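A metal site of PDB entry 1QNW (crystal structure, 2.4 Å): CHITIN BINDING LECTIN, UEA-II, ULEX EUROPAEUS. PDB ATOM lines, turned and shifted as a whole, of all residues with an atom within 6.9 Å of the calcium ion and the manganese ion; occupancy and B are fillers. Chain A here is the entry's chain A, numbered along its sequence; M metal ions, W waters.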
ATOM      1  N   ASP A  86     -18.889   8.147  25.385  1.00  0.00           N
ATOM      2  CA  ASP A  86     -18.645   9.191  24.391  1.00  0.00           C
ATOM      3  C   ASP A  86     -17.161   9.519  24.245  1.00  0.00           C
ATOM      4  O   ASP A  86     -16.729  10.089  23.228  1.00  0.00           O
ATOM      5  CB  ASP A  86     -19.361  10.473  24.803  1.00  0.00           C
ATOM      6  CG  ASP A  86     -20.697  10.639  24.132  1.00  0.00           C
ATOM      7  OD1 ASP A  86     -21.687  10.035  24.588  1.00  0.00           O
ATOM      8  OD2 ASP A  86     -20.745  11.388  23.129  1.00  0.00           O
ATOM      9  N   GLY A  87     -16.396   9.253  25.294  1.00  0.00           N
ATOM     10  CA  GLY A  87     -14.985   9.557  25.226  1.00  0.00           C
ATOM     11  C   GLY A  87     -14.402  10.036  26.544  1.00  0.00           C
ATOM     12  O   GLY A  87     -15.114  10.190  27.541  1.00  0.00           O
ATOM     13  N   ALA A 105     -22.595  14.755  27.638  1.00  0.00           N
ATOM     14  CA  ALA A 105     -21.559  13.748  27.535  1.00  0.00           C
ATOM     15  C   ALA A 105     -20.653  14.000  26.326  1.00  0.00           C
ATOM     16  O   ALA A 105     -19.443  13.775  26.395  1.00  0.00           O
ATOM     17  CB  ALA A 105     -22.172  12.374  27.453  1.00  0.00           C
ATOM     18  N   GLY A 106     -21.258  14.477  25.232  1.00  0.00           N
ATOM     19  CA  GLY A 106     -20.500  14.770  24.022  1.00  0.00           C
ATOM     20  C   GLY A 106     -19.550  15.954  24.148  1.00  0.00           C
ATOM     21  O   GLY A 106     -18.744  16.205  23.259  1.00  0.00           O
ATOM     22  N   MET A 107     -19.682  16.703  25.229  1.00  0.00           N
ATOM     23  CA  MET A 107     -18.832  17.848  25.472  1.00  0.00           C
ATOM     24  C   MET A 107     -17.924  17.578  26.674  1.00  0.00           C
ATOM     25  O   MET A 107     -17.260  18.479  27.190  1.00  0.00           O
ATOM     26  CB  MET A 107     -19.672  19.113  25.677  1.00  0.00           C
ATOM     27  CG  MET A 107     -20.496  19.426  24.444  1.00  0.00           C
ATOM     28  SD  MET A 107     -21.373  20.969  24.518  1.00  0.00           S
ATOM     29  CE  MET A 107     -22.689  20.540  25.668  1.00  0.00           C
ATOM     30  N   PHE A 108     -17.917  16.317  27.108  1.00  0.00           N
ATOM     31  CA  PHE A 108     -17.103  15.824  28.202  1.00  0.00           C
ATOM     32  C   PHE A 108     -17.179  16.624  29.511  1.00  0.00           C
ATOM     33  O   PHE A 108     -16.227  16.645  30.295  1.00  0.00           O
ATOM     34  CB  PHE A 108     -15.649  15.670  27.748  1.00  0.00           C
ATOM     35  CG  PHE A 108     -15.509  14.986  26.416  1.00  0.00           C
ATOM     36  CD1 PHE A 108     -15.865  13.651  26.267  1.00  0.00           C
ATOM     37  CD2 PHE A 108     -15.060  15.698  25.303  1.00  0.00           C
ATOM     38  CE1 PHE A 108     -15.784  13.026  25.024  1.00  0.00           C
ATOM     39  CE2 PHE A 108     -14.976  15.082  24.058  1.00  0.00           C
ATOM     40  CZ  PHE A 108     -15.336  13.751  23.918  1.00  0.00           C
ATOM     41  N   GLU A 126      -8.752  15.438  23.762  1.00  0.00           N
ATOM     42  CA  GLU A 126      -9.838  14.468  23.791  1.00  0.00           C
ATOM     43  C   GLU A 126      -9.564  13.167  23.057  1.00  0.00           C
ATOM     44  O   GLU A 126      -8.859  13.131  22.057  1.00  0.00           O
ATOM     45  CB  GLU A 126     -11.106  15.100  23.225  1.00  0.00           C
ATOM     46  CG  GLU A 126     -10.928  15.624  21.820  1.00  0.00           C
ATOM     47  CD  GLU A 126     -12.232  15.952  21.150  1.00  0.00           C
ATOM     48  OE1 GLU A 126     -13.025  16.739  21.718  1.00  0.00           O
ATOM     49  OE2 GLU A 126     -12.492  15.407  20.062  1.00  0.00           O
ATOM     50  N   PHE A 127     -10.133  12.102  23.591  1.00  0.00           N
ATOM     51  CA  PHE A 127     -10.032  10.777  23.000  1.00  0.00           C
ATOM     52  C   PHE A 127     -11.517  10.477  22.783  1.00  0.00           C
ATOM     53  O   PHE A 127     -12.201   9.929  23.640  1.00  0.00           O
ATOM     54  CB  PHE A 127      -9.351   9.813  23.979  1.00  0.00           C
ATOM     55  CG  PHE A 127      -7.971  10.262  24.381  1.00  0.00           C
ATOM     56  CD1 PHE A 127      -6.855   9.922  23.609  1.00  0.00           C
ATOM     57  CD2 PHE A 127      -7.786  11.098  25.481  1.00  0.00           C
ATOM     58  CE1 PHE A 127      -5.588  10.422  23.916  1.00  0.00           C
ATOM     59  CE2 PHE A 127      -6.512  11.609  25.800  1.00  0.00           C
ATOM     60  CZ  PHE A 127      -5.416  11.262  25.020  1.00  0.00           C
ATOM     61  N   ASP A 128     -12.001  10.998  21.655  1.00  0.00           N
ATOM     62  CA  ASP A 128     -13.397  10.938  21.210  1.00  0.00           C
ATOM     63  C   ASP A 128     -13.825   9.656  20.492  1.00  0.00           C
ATOM     64  O   ASP A 128     -13.430   9.407  19.357  1.00  0.00           O
ATOM     65  CB  ASP A 128     -13.646  12.153  20.310  1.00  0.00           C
ATOM     66  CG  ASP A 128     -15.086  12.573  20.254  1.00  0.00           C
ATOM     67  OD1 ASP A 128     -15.988  11.769  20.560  1.00  0.00           O
ATOM     68  OD2 ASP A 128     -15.324  13.729  19.868  1.00  0.00           O
ATOM     69  N   THR A 129     -14.704   8.885  21.136  1.00  0.00           N
ATOM     70  CA  THR A 129     -15.191   7.615  20.575  1.00  0.00           C
ATOM     71  C   THR A 129     -16.486   7.725  19.766  1.00  0.00           C
ATOM     72  O   THR A 129     -16.822   6.821  18.998  1.00  0.00           O
ATOM     73  CB  THR A 129     -15.403   6.559  21.689  1.00  0.00           C
ATOM     74  OG1 THR A 129     -16.309   7.075  22.677  1.00  0.00           O
ATOM     75  CG2 THR A 129     -14.088   6.183  22.348  1.00  0.00           C
ATOM     76  N   TYR A 130     -17.243   8.808  19.970  1.00  0.00           N
ATOM     77  CA  TYR A 130     -18.502   9.006  19.255  1.00  0.00           C
ATOM     78  C   TYR A 130     -18.423  10.210  18.336  1.00  0.00           C
ATOM     79  O   TYR A 130     -18.162  11.331  18.771  1.00  0.00           O
ATOM     80  CB  TYR A 130     -19.660   9.178  20.253  1.00  0.00           C
ATOM     81  CG  TYR A 130     -20.982   9.492  19.591  1.00  0.00           C
ATOM     82  CD1 TYR A 130     -21.724   8.497  18.949  1.00  0.00           C
ATOM     83  CD2 TYR A 130     -21.484  10.802  19.578  1.00  0.00           C
ATOM     84  CE1 TYR A 130     -22.928   8.797  18.321  1.00  0.00           C
ATOM     85  CE2 TYR A 130     -22.697  11.103  18.945  1.00  0.00           C
ATOM     86  CZ  TYR A 130     -23.404  10.104  18.323  1.00  0.00           C
ATOM     87  OH  TYR A 130     -24.590  10.418  17.688  1.00  0.00           O
ATOM     88  N   PHE A 131     -18.708   9.968  17.064  1.00  0.00           N
ATOM     89  CA  PHE A 131     -18.664  11.020  16.052  1.00  0.00           C
ATOM     90  C   PHE A 131     -19.944  11.109  15.213  1.00  0.00           C
ATOM     91  O   PHE A 131     -19.931  11.678  14.110  1.00  0.00           O
ATOM     92  CB  PHE A 131     -17.454  10.811  15.135  1.00  0.00           C
ATOM     93  CG  PHE A 131     -17.408   9.440  14.508  1.00  0.00           C
ATOM     94  CD1 PHE A 131     -16.853   8.362  15.184  1.00  0.00           C
ATOM     95  CD2 PHE A 131     -17.935   9.233  13.235  1.00  0.00           C
ATOM     96  CE1 PHE A 131     -16.823   7.092  14.606  1.00  0.00           C
ATOM     97  CE2 PHE A 131     -17.911   7.974  12.649  1.00  0.00           C
ATOM     98  CZ  PHE A 131     -17.352   6.898  13.338  1.00  0.00           C
ATOM     99  N   GLY A 132     -21.044  10.549  15.724  1.00  0.00           N
ATOM    100  CA  GLY A 132     -22.306  10.585  14.999  1.00  0.00           C
ATOM    101  C   GLY A 132     -22.737  11.998  14.658  1.00  0.00           C
ATOM    102  O   GLY A 132     -22.800  12.840  15.546  1.00  0.00           O
ATOM    103  N   ASN A 136     -23.113  15.031  17.259  1.00  0.00           N
ATOM    104  CA  ASN A 136     -21.796  15.663  17.202  1.00  0.00           C
ATOM    105  C   ASN A 136     -21.435  16.080  15.783  1.00  0.00           C
ATOM    106  O   ASN A 136     -20.479  15.564  15.199  1.00  0.00           O
ATOM    107  CB  ASN A 136     -20.716  14.708  17.756  1.00  0.00           C
ATOM    108  CG  ASN A 136     -20.826  14.490  19.271  1.00  0.00           C
ATOM    109  OD1 ASN A 136     -20.077  13.696  19.844  1.00  0.00           O
ATOM    110  ND2 ASN A 136     -21.751  15.179  19.901  1.00  0.00           N
ATOM    111  N   TRP A 138     -19.874  18.589  14.739  1.00  0.00           N
ATOM    112  CA  TRP A 138     -18.535  19.186  14.697  1.00  0.00           C
ATOM    113  C   TRP A 138     -17.407  18.166  14.516  1.00  0.00           C
ATOM    114  O   TRP A 138     -16.283  18.532  14.157  1.00  0.00           O
ATOM    115  CB  TRP A 138     -18.280  19.984  15.984  1.00  0.00           C
ATOM    116  CG  TRP A 138     -18.515  19.158  17.224  1.00  0.00           C
ATOM    117  CD1 TRP A 138     -17.674  18.219  17.748  1.00  0.00           C
ATOM    118  CD2 TRP A 138     -19.694  19.143  18.042  1.00  0.00           C
ATOM    119  NE1 TRP A 138     -18.256  17.617  18.852  1.00  0.00           N
ATOM    120  CE2 TRP A 138     -19.491  18.170  19.050  1.00  0.00           C
ATOM    121  CE3 TRP A 138     -20.896  19.858  18.025  1.00  0.00           C
ATOM    122  CZ2 TRP A 138     -20.453  17.889  20.034  1.00  0.00           C
ATOM    123  CZ3 TRP A 138     -21.855  19.587  19.007  1.00  0.00           C
ATOM    124  CH2 TRP A 138     -21.622  18.609  19.985  1.00  0.00           C
ATOM    125  N   ASP A 139     -17.691  16.899  14.768  1.00  0.00           N
ATOM    126  CA  ASP A 139     -16.698  15.821  14.681  1.00  0.00           C
ATOM    127  C   ASP A 139     -16.400  15.282  13.294  1.00  0.00           C
ATOM    128  O   ASP A 139     -17.227  15.377  12.388  1.00  0.00           O
ATOM    129  CB  ASP A 139     -17.137  14.617  15.535  1.00  0.00           C
ATOM    130  CG  ASP A 139     -16.846  14.808  17.000  1.00  0.00           C
ATOM    131  OD1 ASP A 139     -15.962  15.617  17.347  1.00  0.00           O
ATOM    132  OD2 ASP A 139     -17.512  14.138  17.818  1.00  0.00           O
ATOM    133  N   PRO A 140     -15.177  14.726  13.114  1.00  0.00           N
ATOM    134  CA  PRO A 140     -14.751  14.146  11.838  1.00  0.00           C
ATOM    135  C   PRO A 140     -15.415  12.755  11.759  1.00  0.00           C
ATOM    136  O   PRO A 140     -16.042  12.316  12.738  1.00  0.00           O
ATOM    137  CB  PRO A 140     -13.239  14.058  11.983  1.00  0.00           C
ATOM    138  CG  PRO A 140     -13.045  13.906  13.457  1.00  0.00           C
ATOM    139  CD  PRO A 140     -14.024  14.900  14.008  1.00  0.00           C
ATOM    140  N   PHE A 142     -14.606   9.617  12.150  1.00  0.00           N
ATOM    141  CA  PHE A 142     -13.881   8.506  12.752  1.00  0.00           C
ATOM    142  C   PHE A 142     -13.543   8.820  14.205  1.00  0.00           C
ATOM    143  O   PHE A 142     -13.644   9.957  14.640  1.00  0.00           O
ATOM    144  CB  PHE A 142     -12.587   8.221  11.971  1.00  0.00           C
ATOM    145  CG  PHE A 142     -11.791   9.456  11.604  1.00  0.00           C
ATOM    146  CD1 PHE A 142     -11.060  10.148  12.567  1.00  0.00           C
ATOM    147  CD2 PHE A 142     -11.785   9.924  10.296  1.00  0.00           C
ATOM    148  CE1 PHE A 142     -10.335  11.283  12.237  1.00  0.00           C
ATOM    149  CE2 PHE A 142     -11.061  11.066   9.950  1.00  0.00           C
ATOM    150  CZ  PHE A 142     -10.337  11.752  10.924  1.00  0.00           C
ATOM    151  N   HIS A 144     -11.284   9.711  17.119  1.00  0.00           N
ATOM    152  CA  HIS A 144     -10.109  10.559  16.995  1.00  0.00           C
ATOM    153  C   HIS A 144      -9.533  11.129  18.284  1.00  0.00           C
ATOM    154  O   HIS A 144     -10.129  11.054  19.351  1.00  0.00           O
ATOM    155  CB  HIS A 144     -10.486  11.748  16.107  1.00  0.00           C
ATOM    156  CG  HIS A 144     -11.725  12.450  16.558  1.00  0.00           C
ATOM    157  ND1 HIS A 144     -12.982  11.890  16.413  1.00  0.00           N
ATOM    158  CD2 HIS A 144     -11.909  13.620  17.212  1.00  0.00           C
ATOM    159  CE1 HIS A 144     -13.882  12.699  16.949  1.00  0.00           C
ATOM    160  NE2 HIS A 144     -13.257  13.745  17.446  1.00  0.00           N
ATOM    161  N   ILE A 145      -8.351  11.721  18.132  1.00  0.00           N
ATOM    162  CA  ILE A 145      -7.655  12.409  19.211  1.00  0.00           C
ATOM    163  C   ILE A 145      -7.750  13.859  18.750  1.00  0.00           C
ATOM    164  O   ILE A 145      -7.448  14.165  17.597  1.00  0.00           O
ATOM    165  CB  ILE A 145      -6.164  12.010  19.323  1.00  0.00           C
ATOM    166  CG1 ILE A 145      -6.037  10.533  19.667  1.00  0.00           C
ATOM    167  CG2 ILE A 145      -5.478  12.841  20.411  1.00  0.00           C
ATOM    168  CD1 ILE A 145      -4.619  10.041  19.666  1.00  0.00           C
ATOM    169  N   GLY A 146      -8.232  14.740  19.621  1.00  0.00           N
ATOM    170  CA  GLY A 146      -8.349  16.125  19.222  1.00  0.00           C
ATOM    171  C   GLY A 146      -7.768  17.086  20.238  1.00  0.00           C
ATOM    172  O   GLY A 146      -7.704  16.772  21.426  1.00  0.00           O
ATOM    173  N   ASP A 148      -8.470  20.515  21.774  1.00  0.00           N
ATOM    174  CA  ASP A 148      -9.555  21.475  21.929  1.00  0.00           C
ATOM    175  C   ASP A 148      -9.080  22.745  22.606  1.00  0.00           C
ATOM    176  O   ASP A 148      -8.462  22.700  23.654  1.00  0.00           O
ATOM    177  CB  ASP A 148     -10.673  20.868  22.751  1.00  0.00           C
ATOM    178  CG  ASP A 148     -11.250  19.619  22.131  1.00  0.00           C
ATOM    179  OD1 ASP A 148     -10.929  19.309  20.969  1.00  0.00           O
ATOM    180  OD2 ASP A 148     -12.059  18.951  22.798  1.00  0.00           O
ATOM    181  N   ILE A 152     -15.491  22.592  21.641  1.00  0.00           N
ATOM    182  CA  ILE A 152     -15.597  21.143  21.482  1.00  0.00           C
ATOM    183  C   ILE A 152     -15.209  20.761  20.058  1.00  0.00           C
ATOM    184  O   ILE A 152     -14.949  19.599  19.745  1.00  0.00           O
ATOM    185  CB  ILE A 152     -17.031  20.644  21.820  1.00  0.00           C
ATOM    186  CG1 ILE A 152     -17.043  19.119  21.937  1.00  0.00           C
ATOM    187  CG2 ILE A 152     -18.011  21.118  20.762  1.00  0.00           C
ATOM    188  CD1 ILE A 152     -16.130  18.572  23.010  1.00  0.00           C
ATOM    189  N   LYS A 153     -15.175  21.762  19.169  1.00  0.00           N
ATOM    190  CA  LYS A 153     -14.796  21.573  17.784  1.00  0.00           C
ATOM    191  C   LYS A 153     -13.276  21.757  17.740  1.00  0.00           C
ATOM    192  O   LYS A 153     -12.773  22.885  17.738  1.00  0.00           O
ATOM    193  CB  LYS A 153     -15.505  22.613  16.905  1.00  0.00           C
ATOM    194  CG  LYS A 153     -15.179  22.543  15.419  1.00  0.00           C
ATOM    195  CD  LYS A 153     -15.967  23.595  14.637  1.00  0.00           C
ATOM    196  CE  LYS A 153     -15.453  23.745  13.216  1.00  0.00           C
ATOM    197  NZ  LYS A 153     -15.473  22.445  12.501  1.00  0.00           N
ATOM    198  N   SER A 154     -12.551  20.636  17.776  1.00  0.00           N
ATOM    199  CA  SER A 154     -11.089  20.591  17.780  1.00  0.00           C
ATOM    200  C   SER A 154     -10.408  21.432  16.720  1.00  0.00           C
ATOM    201  O   SER A 154     -10.835  21.439  15.561  1.00  0.00           O
ATOM    202  CB  SER A 154     -10.618  19.151  17.621  1.00  0.00           C
ATOM    203  OG  SER A 154     -11.285  18.287  18.517  1.00  0.00           O
ATOM    204  N   THR A 157      -7.302  17.389  14.674  1.00  0.00           N
ATOM    205  CA  THR A 157      -7.595  16.006  15.052  1.00  0.00           C
ATOM    206  C   THR A 157      -6.732  15.047  14.253  1.00  0.00           C
ATOM    207  O   THR A 157      -6.093  15.431  13.280  1.00  0.00           O
ATOM    208  CB  THR A 157      -9.070  15.620  14.802  1.00  0.00           C
ATOM    209  OG1 THR A 157      -9.331  15.681  13.399  1.00  0.00           O
ATOM    210  CG2 THR A 157     -10.027  16.518  15.549  1.00  0.00           C
HETATM  211 CA    CA M   1     -17.815  13.159  20.013  1.00  0.00          CA
HETATM  212 MN    MN M   2     -14.283  15.143  18.766  1.00  0.00          MN
HETATM  213  O   HOH W   1     -15.274  16.780  20.059  1.00  0.00           O
HETATM  214  O   HOH W   2     -17.676  15.363  20.942  1.00  0.00           O
HETATM  215  O   HOH W   3     -13.425  16.587  17.758  1.00  0.00           O
HETATM  216  O   HOH W   4     -18.226  11.980  22.010  1.00  0.00           O
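OE2 of Glu 126 lies close to OG of Ser 154 (3.5 Å).
The side-chain carboxylate (OD1) of Asp 139 sits close to the indole nitrogen (NE1) of Trp 138 (3.4 Å).
OE1 of Glu 126 sits close to OD2 of Asp 148, 2.6 Å away.
O of Gly 146 lies within hydrogen-bond range of N of Glu 126 (2.9 Å).
ND1 of His 144 sits at hydrogen-bond distance from O of Phe 142, at 2.7 Å.
Of the 26 residues printed, 4 come within 4 Å of the calcium ion.
Within 4 Å of the manganese ion: Glu 126, Asp 128, Asp 139 and His 144.
The nearest printed residue that does not touch the manganese ion is Ser 154 (4.4 Å).
The calcium ion is bound by O of Tyr 130, OD1 of Asn 136, water W4, OD1 of Asp 128, water W2, OD2 of Asp 139 and OD2 of Asp 128.
The manganese ion is bound by water W3 (2.0 Å), OD2 of Asp 128 (2.1 Å), NE2 of His 144 (2.2 Å), OE2 of Glu 126 (2.2 Å), OD1 of Asp 139 (2.2 Å) and water W1 (2.3 Å).
The manganese ion has six donor atoms within binding distance.
Water W2 bridges O of Gly 106 and NE1 of Trp 138.
Water W1 lies within hydrogen-bond range of the side-chain carboxylate of Glu 126, the backbone carbonyl oxygen of Ile 152 and the indole nitrogen of Trp 138.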
